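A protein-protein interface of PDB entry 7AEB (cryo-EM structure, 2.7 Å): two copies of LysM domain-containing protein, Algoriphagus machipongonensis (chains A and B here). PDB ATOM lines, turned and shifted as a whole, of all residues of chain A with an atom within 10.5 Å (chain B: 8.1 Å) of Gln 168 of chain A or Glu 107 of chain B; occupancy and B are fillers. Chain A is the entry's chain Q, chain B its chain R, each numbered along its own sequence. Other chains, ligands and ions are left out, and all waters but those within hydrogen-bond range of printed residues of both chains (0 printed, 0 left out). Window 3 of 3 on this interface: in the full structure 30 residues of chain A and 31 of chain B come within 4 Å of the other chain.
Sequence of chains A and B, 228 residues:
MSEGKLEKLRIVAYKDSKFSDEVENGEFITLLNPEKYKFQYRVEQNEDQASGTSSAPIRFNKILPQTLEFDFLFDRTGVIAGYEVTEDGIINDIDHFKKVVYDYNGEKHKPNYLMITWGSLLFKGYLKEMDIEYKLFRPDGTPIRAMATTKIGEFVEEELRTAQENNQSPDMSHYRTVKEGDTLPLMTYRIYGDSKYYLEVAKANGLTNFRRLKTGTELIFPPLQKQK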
ATOM      1  N   THR A 162      13.112 -10.334  -7.542  1.00  0.00           N
ATOM      2  CA  THR A 162      14.375  -9.922  -6.945  1.00  0.00           C
ATOM      3  C   THR A 162      15.311  -9.248  -7.942  1.00  0.00           C
ATOM      4  O   THR A 162      16.168  -8.468  -7.525  1.00  0.00           O
ATOM      5  CB  THR A 162      15.080 -11.120  -6.310  1.00  0.00           C
ATOM      6  OG1 THR A 162      15.240 -12.158  -7.282  1.00  0.00           O
ATOM      7  CG2 THR A 162      14.281 -11.655  -5.144  1.00  0.00           C
ATOM      8  N   ALA A 163      15.170  -9.516  -9.238  1.00  0.00           N
ATOM      9  CA  ALA A 163      15.987  -8.817 -10.222  1.00  0.00           C
ATOM     10  C   ALA A 163      15.450  -7.421 -10.511  1.00  0.00           C
ATOM     11  O   ALA A 163      16.214  -6.533 -10.896  1.00  0.00           O
ATOM     12  CB  ALA A 163      16.065  -9.634 -11.508  1.00  0.00           C
ATOM     13  N   GLN A 164      14.146  -7.210 -10.335  1.00  0.00           N
ATOM     14  CA  GLN A 164      13.569  -5.884 -10.518  1.00  0.00           C
ATOM     15  C   GLN A 164      13.739  -5.027  -9.270  1.00  0.00           C
ATOM     16  O   GLN A 164      13.920  -3.812  -9.370  1.00  0.00           O
ATOM     17  CB  GLN A 164      12.091  -6.001 -10.893  1.00  0.00           C
ATOM     18  CG  GLN A 164      11.854  -6.453 -12.315  1.00  0.00           C
ATOM     19  CD  GLN A 164      10.419  -6.862 -12.577  1.00  0.00           C
ATOM     20  OE1 GLN A 164       9.790  -7.528 -11.763  1.00  0.00           O
ATOM     21  NE2 GLN A 164       9.899  -6.462 -13.725  1.00  0.00           N
ATOM     22  N   GLU A 165      13.668  -5.643  -8.092  1.00  0.00           N
ATOM     23  CA  GLU A 165      14.033  -4.999  -6.832  1.00  0.00           C
ATOM     24  C   GLU A 165      15.515  -5.247  -6.598  1.00  0.00           C
ATOM     25  O   GLU A 165      15.919  -6.137  -5.846  1.00  0.00           O
ATOM     26  CB  GLU A 165      13.213  -5.555  -5.678  1.00  0.00           C
ATOM     27  CG  GLU A 165      11.732  -5.358  -5.788  1.00  0.00           C
ATOM     28  CD  GLU A 165      10.974  -6.129  -4.733  1.00  0.00           C
ATOM     29  OE1 GLU A 165      11.613  -6.818  -3.913  1.00  0.00           O
ATOM     30  OE2 GLU A 165       9.727  -6.047  -4.724  1.00  0.00           O
ATOM     31  N   ASN A 166      16.344  -4.448  -7.258  1.00  0.00           N
ATOM     32  CA  ASN A 166      17.795  -4.589  -7.140  1.00  0.00           C
ATOM     33  C   ASN A 166      18.202  -4.036  -5.773  1.00  0.00           C
ATOM     34  O   ASN A 166      18.641  -2.893  -5.621  1.00  0.00           O
ATOM     35  CB  ASN A 166      18.486  -3.888  -8.305  1.00  0.00           C
ATOM     36  CG  ASN A 166      19.987  -3.908  -8.202  1.00  0.00           C
ATOM     37  OD1 ASN A 166      20.587  -4.892  -7.779  1.00  0.00           O
ATOM     38  ND2 ASN A 166      20.608  -2.804  -8.578  1.00  0.00           N
ATOM     39  N   ASN A 167      18.027  -4.871  -4.752  1.00  0.00           N
ATOM     40  CA  ASN A 167      18.173  -4.453  -3.365  1.00  0.00           C
ATOM     41  C   ASN A 167      19.648  -4.326  -3.013  1.00  0.00           C
ATOM     42  O   ASN A 167      20.403  -5.296  -3.113  1.00  0.00           O
ATOM     43  CB  ASN A 167      17.481  -5.449  -2.441  1.00  0.00           C
ATOM     44  CG  ASN A 167      16.005  -5.181  -2.307  1.00  0.00           C
ATOM     45  OD1 ASN A 167      15.580  -4.036  -2.229  1.00  0.00           O
ATOM     46  ND2 ASN A 167      15.213  -6.236  -2.295  1.00  0.00           N
ATOM     47  N   GLN A 168      20.058  -3.136  -2.605  1.00  0.00           N
ATOM     48  CA  GLN A 168      21.450  -2.909  -2.253  1.00  0.00           C
ATOM     49  C   GLN A 168      21.588  -2.376  -0.835  1.00  0.00           C
ATOM     50  O   GLN A 168      21.707  -3.148   0.119  1.00  0.00           O
ATOM     51  CB  GLN A 168      22.093  -1.949  -3.247  1.00  0.00           C
ATOM     52  CG  GLN A 168      21.819  -0.495  -2.976  1.00  0.00           C
ATOM     53  CD  GLN A 168      21.930   0.343  -4.224  1.00  0.00           C
ATOM     54  OE1 GLN A 168      21.488  -0.064  -5.296  1.00  0.00           O
ATOM     55  NE2 GLN A 168      22.524   1.521  -4.095  1.00  0.00           N
ATOM     56  N   PRO A 170      25.598  -0.681   3.003  1.00  0.00           N
ATOM     57  CA  PRO A 170      25.952  -1.490   4.172  1.00  0.00           C
ATOM     58  C   PRO A 170      25.913  -2.999   3.933  1.00  0.00           C
ATOM     59  O   PRO A 170      26.280  -3.741   4.835  1.00  0.00           O
ATOM     60  CB  PRO A 170      24.898  -1.078   5.201  1.00  0.00           C
ATOM     61  CG  PRO A 170      24.575   0.310   4.852  1.00  0.00           C
ATOM     62  CD  PRO A 170      24.688   0.421   3.359  1.00  0.00           C
ATOM     63  N   ASP A 171      25.475  -3.450   2.757  1.00  0.00           N
ATOM     64  CA  ASP A 171      25.547  -4.865   2.414  1.00  0.00           C
ATOM     65  C   ASP A 171      26.431  -5.167   1.215  1.00  0.00           C
ATOM     66  O   ASP A 171      26.952  -6.281   1.120  1.00  0.00           O
ATOM     67  CB  ASP A 171      24.151  -5.436   2.144  1.00  0.00           C
ATOM     68  CG  ASP A 171      23.395  -5.765   3.407  1.00  0.00           C
ATOM     69  OD1 ASP A 171      24.042  -6.127   4.409  1.00  0.00           O
ATOM     70  OD2 ASP A 171      22.152  -5.678   3.402  1.00  0.00           O
ATOM     71  N   MET A 172      26.620  -4.223   0.299  1.00  0.00           N
ATOM     72  CA  MET A 172      27.402  -4.460  -0.907  1.00  0.00           C
ATOM     73  C   MET A 172      28.612  -3.538  -0.942  1.00  0.00           C
ATOM     74  O   MET A 172      28.813  -2.711  -0.053  1.00  0.00           O
ATOM     75  CB  MET A 172      26.562  -4.256  -2.174  1.00  0.00           C
ATOM     76  CG  MET A 172      25.101  -4.667  -2.063  1.00  0.00           C
ATOM     77  SD  MET A 172      24.834  -6.424  -1.762  1.00  0.00           S
ATOM     78  CE  MET A 172      25.649  -7.131  -3.176  1.00  0.00           C
ATOM     79  N   SER A 173      29.414  -3.688  -1.989  1.00  0.00           N
ATOM     80  CA  SER A 173      30.603  -2.869  -2.176  1.00  0.00           C
ATOM     81  C   SER A 173      30.327  -1.705  -3.123  1.00  0.00           C
ATOM     82  O   SER A 173      29.440  -1.759  -3.972  1.00  0.00           O
ATOM     83  CB  SER A 173      31.747  -3.712  -2.723  1.00  0.00           C
ATOM     84  OG  SER A 173      32.252  -4.571  -1.728  1.00  0.00           O
ATOM     85  N   HIS A 174      31.127  -0.648  -2.980  1.00  0.00           N
ATOM     86  CA  HIS A 174      30.901   0.602  -3.690  1.00  0.00           C
ATOM     87  C   HIS A 174      32.238   1.254  -4.010  1.00  0.00           C
ATOM     88  O   HIS A 174      33.217   1.052  -3.293  1.00  0.00           O
ATOM     89  CB  HIS A 174      30.030   1.535  -2.845  1.00  0.00           C
ATOM     90  CG  HIS A 174      29.616   2.787  -3.550  1.00  0.00           C
ATOM     91  ND1 HIS A 174      28.936   2.778  -4.746  1.00  0.00           N
ATOM     92  CD2 HIS A 174      29.790   4.088  -3.227  1.00  0.00           C
ATOM     93  CE1 HIS A 174      28.710   4.019  -5.133  1.00  0.00           C
ATOM     94  NE2 HIS A 174      29.216   4.833  -4.227  1.00  0.00           N
ATOM     95  N   TYR A 175      32.287   2.019  -5.104  1.00  0.00           N
ATOM     96  CA  TYR A 175      33.457   2.827  -5.432  1.00  0.00           C
ATOM     97  C   TYR A 175      33.023   4.211  -5.905  1.00  0.00           C
ATOM     98  O   TYR A 175      31.978   4.368  -6.538  1.00  0.00           O
ATOM     99  CB  TYR A 175      34.369   2.139  -6.489  1.00  0.00           C
ATOM    100  CG  TYR A 175      33.744   1.825  -7.836  1.00  0.00           C
ATOM    101  CD1 TYR A 175      33.705   2.775  -8.850  1.00  0.00           C
ATOM    102  CD2 TYR A 175      33.233   0.566  -8.107  1.00  0.00           C
ATOM    103  CE1 TYR A 175      33.141   2.496 -10.071  1.00  0.00           C
ATOM    104  CE2 TYR A 175      32.669   0.275  -9.333  1.00  0.00           C
ATOM    105  CZ  TYR A 175      32.624   1.244 -10.307  1.00  0.00           C
ATOM    106  OH  TYR A 175      32.068   0.962 -11.530  1.00  0.00           O
ATOM    107  N   ARG A 176      33.832   5.219  -5.573  1.00  0.00           N
ATOM    108  CA  ARG A 176      33.639   6.590  -6.031  1.00  0.00           C
ATOM    109  C   ARG A 176      34.975   7.178  -6.455  1.00  0.00           C
ATOM    110  O   ARG A 176      36.041   6.659  -6.121  1.00  0.00           O
ATOM    111  CB  ARG A 176      33.040   7.509  -4.955  1.00  0.00           C
ATOM    112  CG  ARG A 176      31.803   7.013  -4.270  1.00  0.00           C
ATOM    113  CD  ARG A 176      31.207   8.084  -3.408  1.00  0.00           C
ATOM    114  NE  ARG A 176      30.366   8.976  -4.187  1.00  0.00           N
ATOM    115  CZ  ARG A 176      29.065   8.804  -4.372  1.00  0.00           C
ATOM    116  NH1 ARG A 176      28.448   7.767  -3.827  1.00  0.00           N
ATOM    117  NH2 ARG A 176      28.381   9.670  -5.101  1.00  0.00           N
ATOM    118  N   MET A 187      31.214  12.055   2.888  1.00  0.00           N
ATOM    119  CA  MET A 187      30.953  10.956   1.964  1.00  0.00           C
ATOM    120  C   MET A 187      30.556   9.686   2.701  1.00  0.00           C
ATOM    121  O   MET A 187      29.774   8.885   2.183  1.00  0.00           O
ATOM    122  CB  MET A 187      32.181  10.691   1.094  1.00  0.00           C
ATOM    123  CG  MET A 187      32.435  11.723   0.026  1.00  0.00           C
ATOM    124  SD  MET A 187      33.619  11.160  -1.209  1.00  0.00           S
ATOM    125  CE  MET A 187      35.095  10.998  -0.224  1.00  0.00           C
ATOM    126  N   TYR A 189      28.820   9.594   5.435  1.00  0.00           N
ATOM    127  CA  TYR A 189      27.447   9.776   5.886  1.00  0.00           C
ATOM    128  C   TYR A 189      26.443   9.458   4.785  1.00  0.00           C
ATOM    129  O   TYR A 189      25.360   8.931   5.055  1.00  0.00           O
ATOM    130  CB  TYR A 189      27.264  11.210   6.378  1.00  0.00           C
ATOM    131  CG  TYR A 189      25.858  11.554   6.760  1.00  0.00           C
ATOM    132  CD1 TYR A 189      25.274  11.000   7.887  1.00  0.00           C
ATOM    133  CD2 TYR A 189      25.104  12.424   5.983  1.00  0.00           C
ATOM    134  CE1 TYR A 189      23.982  11.310   8.242  1.00  0.00           C
ATOM    135  CE2 TYR A 189      23.812  12.738   6.328  1.00  0.00           C
ATOM    136  CZ  TYR A 189      23.258  12.182   7.461  1.00  0.00           C
ATOM    137  OH  TYR A 189      21.969  12.497   7.813  1.00  0.00           O
ATOM    138  N   ARG A 190      26.781   9.773   3.537  1.00  0.00           N
ATOM    139  CA  ARG A 190      25.846   9.545   2.447  1.00  0.00           C
ATOM    140  C   ARG A 190      25.822   8.094   1.996  1.00  0.00           C
ATOM    141  O   ARG A 190      24.891   7.682   1.299  1.00  0.00           O
ATOM    142  CB  ARG A 190      26.192  10.448   1.266  1.00  0.00           C
ATOM    143  CG  ARG A 190      25.841  11.891   1.491  1.00  0.00           C
ATOM    144  CD  ARG A 190      26.448  12.782   0.436  1.00  0.00           C
ATOM    145  NE  ARG A 190      26.038  14.169   0.613  1.00  0.00           N
ATOM    146  CZ  ARG A 190      26.465  15.180  -0.138  1.00  0.00           C
ATOM    147  NH1 ARG A 190      27.315  14.961  -1.127  1.00  0.00           N
ATOM    148  NH2 ARG A 190      26.036  16.407   0.098  1.00  0.00           N
ATOM    149  N   ILE A 191      26.821   7.307   2.371  1.00  0.00           N
ATOM    150  CA  ILE A 191      26.894   5.922   1.941  1.00  0.00           C
ATOM    151  C   ILE A 191      26.400   4.979   3.032  1.00  0.00           C
ATOM    152  O   ILE A 191      25.668   4.026   2.760  1.00  0.00           O
ATOM    153  CB  ILE A 191      28.338   5.601   1.489  1.00  0.00           C
ATOM    154  CG1 ILE A 191      28.640   6.335   0.181  1.00  0.00           C
ATOM    155  CG2 ILE A 191      28.561   4.120   1.301  1.00  0.00           C
ATOM    156  CD1 ILE A 191      30.089   6.399  -0.166  1.00  0.00           C
ATOM    157  N   TYR A 192      26.736   5.262   4.287  1.00  0.00           N
ATOM    158  CA  TYR A 192      26.372   4.390   5.392  1.00  0.00           C
ATOM    159  C   TYR A 192      25.229   4.920   6.244  1.00  0.00           C
ATOM    160  O   TYR A 192      24.584   4.131   6.937  1.00  0.00           O
ATOM    161  CB  TYR A 192      27.581   4.145   6.301  1.00  0.00           C
ATOM    162  CG  TYR A 192      28.717   3.418   5.633  1.00  0.00           C
ATOM    163  CD1 TYR A 192      28.659   2.049   5.428  1.00  0.00           C
ATOM    164  CD2 TYR A 192      29.846   4.099   5.208  1.00  0.00           C
ATOM    165  CE1 TYR A 192      29.689   1.379   4.814  1.00  0.00           C
ATOM    166  CE2 TYR A 192      30.883   3.434   4.598  1.00  0.00           C
ATOM    167  CZ  TYR A 192      30.796   2.076   4.402  1.00  0.00           C
ATOM    168  OH  TYR A 192      31.825   1.404   3.795  1.00  0.00           O
ATOM    169  N   GLY A 193      24.964   6.219   6.219  1.00  0.00           N
ATOM    170  CA  GLY A 193      24.014   6.804   7.135  1.00  0.00           C
ATOM    171  C   GLY A 193      24.603   7.313   8.430  1.00  0.00           C
ATOM    172  O   GLY A 193      23.848   7.772   9.290  1.00  0.00           O
ATOM    173  N   PRO A 223      31.451  -3.246   2.681  1.00  0.00           N
ATOM    174  CA  PRO A 223      30.253  -3.399   3.508  1.00  0.00           C
ATOM    175  C   PRO A 223      30.595  -3.710   4.958  1.00  0.00           C
ATOM    176  O   PRO A 223      31.710  -4.101   5.297  1.00  0.00           O
ATOM    177  CB  PRO A 223      29.528  -4.576   2.853  1.00  0.00           C
ATOM    178  CG  PRO A 223      30.610  -5.366   2.250  1.00  0.00           C
ATOM    179  CD  PRO A 223      31.610  -4.377   1.750  1.00  0.00           C
ATOM    180  N   LEU A 224      29.604  -3.531   5.819  1.00  0.00           N
ATOM    181  CA  LEU A 224      29.733  -3.848   7.232  1.00  0.00           C
ATOM    182  C   LEU A 224      29.608  -5.349   7.457  1.00  0.00           C
ATOM    183  O   LEU A 224      28.887  -6.044   6.736  1.00  0.00           O
ATOM    184  CB  LEU A 224      28.664  -3.113   8.038  1.00  0.00           C
ATOM    185  CG  LEU A 224      28.646  -1.595   7.864  1.00  0.00           C
ATOM    186  CD1 LEU A 224      27.474  -0.983   8.585  1.00  0.00           C
ATOM    187  CD2 LEU A 224      29.942  -0.997   8.353  1.00  0.00           C
ATOM    188  N   LYS A 226      28.505  -8.865   9.272  1.00  0.00           N
ATOM    189  CA  LYS A 226      27.131  -9.229   9.604  1.00  0.00           C
ATOM    190  C   LYS A 226      26.986  -9.950  10.935  1.00  0.00           C
ATOM    191  O   LYS A 226      26.029  -9.685  11.670  1.00  0.00           O
ATOM    192  CB  LYS A 226      26.541 -10.089   8.488  1.00  0.00           C
ATOM    193  CG  LYS A 226      26.188  -9.296   7.249  1.00  0.00           C
ATOM    194  CD  LYS A 226      25.316 -10.090   6.300  1.00  0.00           C
ATOM    195  CE  LYS A 226      26.081 -11.233   5.663  1.00  0.00           C
ATOM    196  NZ  LYS A 226      25.612 -11.481   4.273  1.00  0.00           N
ATOM    197  N   LYS B  15      15.119  11.226  -1.440  1.00  0.00           N
ATOM    198  CA  LYS B  15      15.731  10.021  -0.887  1.00  0.00           C
ATOM    199  C   LYS B  15      15.686   9.929   0.629  1.00  0.00           C
ATOM    200  O   LYS B  15      15.606   8.821   1.163  1.00  0.00           O
ATOM    201  CB  LYS B  15      17.194   9.910  -1.322  1.00  0.00           C
ATOM    202  CG  LYS B  15      17.402   9.480  -2.753  1.00  0.00           C
ATOM    203  CD  LYS B  15      18.866   9.255  -3.037  1.00  0.00           C
ATOM    204  CE  LYS B  15      19.597  10.576  -3.139  1.00  0.00           C
ATOM    205  NZ  LYS B  15      21.018  10.403  -3.517  1.00  0.00           N
ATOM    206  N   GLU B  22      17.920  14.861  -3.580  1.00  0.00           N
ATOM    207  CA  GLU B  22      16.988  14.586  -4.664  1.00  0.00           C
ATOM    208  C   GLU B  22      17.340  13.308  -5.414  1.00  0.00           C
ATOM    209  O   GLU B  22      18.510  12.992  -5.635  1.00  0.00           O
ATOM    210  CB  GLU B  22      16.955  15.746  -5.652  1.00  0.00           C
ATOM    211  CG  GLU B  22      16.364  17.014  -5.098  1.00  0.00           C
ATOM    212  CD  GLU B  22      16.269  18.104  -6.138  1.00  0.00           C
ATOM    213  OE1 GLU B  22      16.133  17.776  -7.334  1.00  0.00           O
ATOM    214  OE2 GLU B  22      16.339  19.293  -5.764  1.00  0.00           O
ATOM    215  N   VAL B  23      16.299  12.582  -5.810  1.00  0.00           N
ATOM    216  CA  VAL B  23      16.429  11.479  -6.752  1.00  0.00           C
ATOM    217  C   VAL B  23      16.775  12.059  -8.117  1.00  0.00           C
ATOM    218  O   VAL B  23      16.200  13.068  -8.538  1.00  0.00           O
ATOM    219  CB  VAL B  23      15.121  10.660  -6.787  1.00  0.00           C
ATOM    220  CG1 VAL B  23      15.073   9.682  -7.958  1.00  0.00           C
ATOM    221  CG2 VAL B  23      14.917   9.925  -5.487  1.00  0.00           C
ATOM    222  N   GLU B  24      17.742  11.453  -8.800  1.00  0.00           N
ATOM    223  CA  GLU B  24      18.166  11.964 -10.095  1.00  0.00           C
ATOM    224  C   GLU B  24      17.154  11.603 -11.176  1.00  0.00           C
ATOM    225  O   GLU B  24      16.727  10.449 -11.273  1.00  0.00           O
ATOM    226  CB  GLU B  24      19.546  11.421 -10.447  1.00  0.00           C
ATOM    227  CG  GLU B  24      20.644  11.941  -9.538  1.00  0.00           C
ATOM    228  CD  GLU B  24      20.885  13.433  -9.700  1.00  0.00           C
ATOM    229  OE1 GLU B  24      20.730  13.948 -10.827  1.00  0.00           O
ATOM    230  OE2 GLU B  24      21.228  14.093  -8.696  1.00  0.00           O
ATOM    231  N   TYR B 104       9.161   1.088  -6.977  1.00  0.00           N
ATOM    232  CA  TYR B 104      10.010   0.699  -5.860  1.00  0.00           C
ATOM    233  C   TYR B 104      11.466   1.052  -6.162  1.00  0.00           C
ATOM    234  O   TYR B 104      11.954   0.827  -7.269  1.00  0.00           O
ATOM    235  CB  TYR B 104       9.823  -0.803  -5.620  1.00  0.00           C
ATOM    236  CG  TYR B 104      10.562  -1.488  -4.484  1.00  0.00           C
ATOM    237  CD1 TYR B 104       9.897  -1.853  -3.323  1.00  0.00           C
ATOM    238  CD2 TYR B 104      11.898  -1.858  -4.611  1.00  0.00           C
ATOM    239  CE1 TYR B 104      10.552  -2.517  -2.307  1.00  0.00           C
ATOM    240  CE2 TYR B 104      12.559  -2.498  -3.602  1.00  0.00           C
ATOM    241  CZ  TYR B 104      11.886  -2.833  -2.457  1.00  0.00           C
ATOM    242  OH  TYR B 104      12.564  -3.484  -1.462  1.00  0.00           O
ATOM    243  N   ASN B 105      12.160   1.597  -5.171  1.00  0.00           N
ATOM    244  CA  ASN B 105      13.542   2.040  -5.310  1.00  0.00           C
ATOM    245  C   ASN B 105      14.432   1.083  -4.527  1.00  0.00           C
ATOM    246  O   ASN B 105      14.294   0.958  -3.308  1.00  0.00           O
ATOM    247  CB  ASN B 105      13.691   3.476  -4.802  1.00  0.00           C
ATOM    248  CG  ASN B 105      14.933   4.168  -5.319  1.00  0.00           C
ATOM    249  OD1 ASN B 105      15.852   3.534  -5.826  1.00  0.00           O
ATOM    250  ND2 ASN B 105      14.965   5.484  -5.187  1.00  0.00           N
ATOM    251  N   GLY B 106      15.336   0.401  -5.230  1.00  0.00           N
ATOM    252  CA  GLY B 106      16.197  -0.589  -4.606  1.00  0.00           C
ATOM    253  C   GLY B 106      17.314  -0.013  -3.766  1.00  0.00           C
ATOM    254  O   GLY B 106      17.932  -0.754  -2.997  1.00  0.00           O
ATOM    255  N   GLU B 107      17.579   1.285  -3.886  1.00  0.00           N
ATOM    256  CA  GLU B 107      18.579   1.921  -3.038  1.00  0.00           C
ATOM    257  C   GLU B 107      18.065   2.126  -1.619  1.00  0.00           C
ATOM    258  O   GLU B 107      18.843   2.056  -0.662  1.00  0.00           O
ATOM    259  CB  GLU B 107      18.999   3.249  -3.655  1.00  0.00           C
ATOM    260  CG  GLU B 107      20.317   3.775  -3.153  1.00  0.00           C
ATOM    261  CD  GLU B 107      20.519   5.224  -3.510  1.00  0.00           C
ATOM    262  OE1 GLU B 107      19.843   5.698  -4.447  1.00  0.00           O
ATOM    263  OE2 GLU B 107      21.354   5.888  -2.866  1.00  0.00           O
ATOM    264  N   LYS B 108      16.767   2.387  -1.461  1.00  0.00           N
ATOM    265  CA  LYS B 108      16.175   2.638  -0.156  1.00  0.00           C
ATOM    266  C   LYS B 108      15.192   1.570   0.291  1.00  0.00           C
ATOM    267  O   LYS B 108      14.665   1.684   1.401  1.00  0.00           O
ATOM    268  CB  LYS B 108      15.464   3.995  -0.146  1.00  0.00           C
ATOM    269  CG  LYS B 108      16.380   5.176  -0.336  1.00  0.00           C
ATOM    270  CD  LYS B 108      17.382   5.292   0.794  1.00  0.00           C
ATOM    271  CE  LYS B 108      18.505   6.232   0.411  1.00  0.00           C
ATOM    272  NZ  LYS B 108      19.559   6.308   1.452  1.00  0.00           N
ATOM    273  N   HIS B 109      14.922   0.563  -0.551  1.00  0.00           N
ATOM    274  CA  HIS B 109      14.023  -0.567  -0.273  1.00  0.00           C
ATOM    275  C   HIS B 109      12.574  -0.128  -0.051  1.00  0.00           C
ATOM    276  O   HIS B 109      11.861  -0.731   0.747  1.00  0.00           O
ATOM    277  CB  HIS B 109      14.505  -1.420   0.911  1.00  0.00           C
ATOM    278  CG  HIS B 109      15.966  -1.742   0.884  1.00  0.00           C
ATOM    279  ND1 HIS B 109      16.457  -2.925   0.384  1.00  0.00           N
ATOM    280  CD2 HIS B 109      17.040  -1.044   1.316  1.00  0.00           C
ATOM    281  CE1 HIS B 109      17.772  -2.936   0.496  1.00  0.00           C
ATOM    282  NE2 HIS B 109      18.151  -1.804   1.053  1.00  0.00           N
ATOM    283  N   LYS B 110      12.124   0.899  -0.783  1.00  0.00           N
ATOM    284  CA  LYS B 110      10.792   1.482  -0.624  1.00  0.00           C
ATOM    285  C   LYS B 110      10.459   2.378  -1.815  1.00  0.00           C
ATOM    286  O   LYS B 110      11.334   2.633  -2.647  1.00  0.00           O
ATOM    287  CB  LYS B 110      10.721   2.274   0.684  1.00  0.00           C
ATOM    288  CG  LYS B 110      11.858   3.240   0.847  1.00  0.00           C
ATOM    289  CD  LYS B 110      11.994   3.724   2.260  1.00  0.00           C
ATOM    290  CE  LYS B 110      11.099   4.886   2.504  1.00  0.00           C
ATOM    291  NZ  LYS B 110      11.520   6.047   1.676  1.00  0.00           N
ATOM    292  N   ASN B 112       9.337   6.327  -3.171  1.00  0.00           N
ATOM    293  CA  ASN B 112       9.991   7.612  -2.930  1.00  0.00           C
ATOM    294  C   ASN B 112       9.184   8.518  -1.994  1.00  0.00           C
ATOM    295  O   ASN B 112       7.966   8.410  -1.871  1.00  0.00           O
ATOM    296  CB  ASN B 112      10.220   8.343  -4.255  1.00  0.00           C
ATOM    297  CG  ASN B 112      11.331   7.725  -5.089  1.00  0.00           C
ATOM    298  OD1 ASN B 112      12.286   7.179  -4.559  1.00  0.00           O
ATOM    299  ND2 ASN B 112      11.209   7.826  -6.401  1.00  0.00           N
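Ala 163 of chain A touches none of the printed residues of chain B. Of the printed residues of chain B, Glu 165 of chain A touches Tyr 104. Of the printed residues of chain B, Asn 166 of chain A touches Gly 106 (3.5 Å). Printed residues of chain B within 4 Å of Asn 167 of chain A: Tyr 104 (3.2 Å), Gly 106 (3.7 Å) and His 109 (3.0 Å). Printed residues of chain B within 4 Å of Gln 168 of chain A: Gly 106 (3.2 Å), Glu 107 (3.3 Å) and His 109 (3.9 Å). Of the printed residues of chain A, Tyr 104 of chain B touches Glu 165 (3.7 Å) and Asn 167 (3.2 Å). No residue of chain A comes within 4 Å of Asn 105 of chain B. Of chain A, only Asn 166 (3.5 Å), Asn 167 (3.7 Å) and Gln 168 (3.2 Å) come within 4 Å of Gly 106 of chain B. Glu 107 of chain B touches just one residue of chain A: Gln 168 (3.3 Å). Printed residues of chain A within 4 Å of His 109 of chain B: Asn 167 (3.0 Å) and Gln 168 (3.9 Å). The nearest residue of chain B that does not touch Gln 168 of chain A is Lys 108 of chain B (6.0 Å).
Hydrophobic or aromatic side chains of chain B that line the printed part of chain A: Tyr 104 and His 109. Among the printed residues, 8 pairs touch across the chains.
Among the printed residues, pairs that only touch across the chains: Gln 168 of chain A with Glu 107 of chain B (3.3 Å), Glu 165 of chain A with Tyr 104 of chain B (3.7 Å), Asn 167 of chain A with Gly 106 of chain B (3.7 Å) and Gln 168 of chain A with His 109 of chain B (3.9 Å).
No position is printed for both chains. Of the 8 pairs that touch across the chains among the printed residues, none has its exchanged pair printed and touching as well.
The side-chain amide oxygen (OD1) of Asn 167 of chain A lies within hydrogen-bond range of the side-chain hydroxyl (OH) of Tyr 104 of chain B, at 3.2 Å. ND1 of His 109 of chain B sits at hydrogen-bond distance from OD1 of Asn 167 of chain A, 3.0 Å away. The backbone carbonyl oxygen (O) of Gly 106 of chain B is in hydrogen-bond range of the backbone NH (N) of Gln 168 of chain A, 3.2 Å away. O of Gly 106 of chain B lies close to O of Asn 166 of chain A (3.5 Å).
N of Glu 107 of chain B lies close to OD1 of Asn 105 of chain B.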
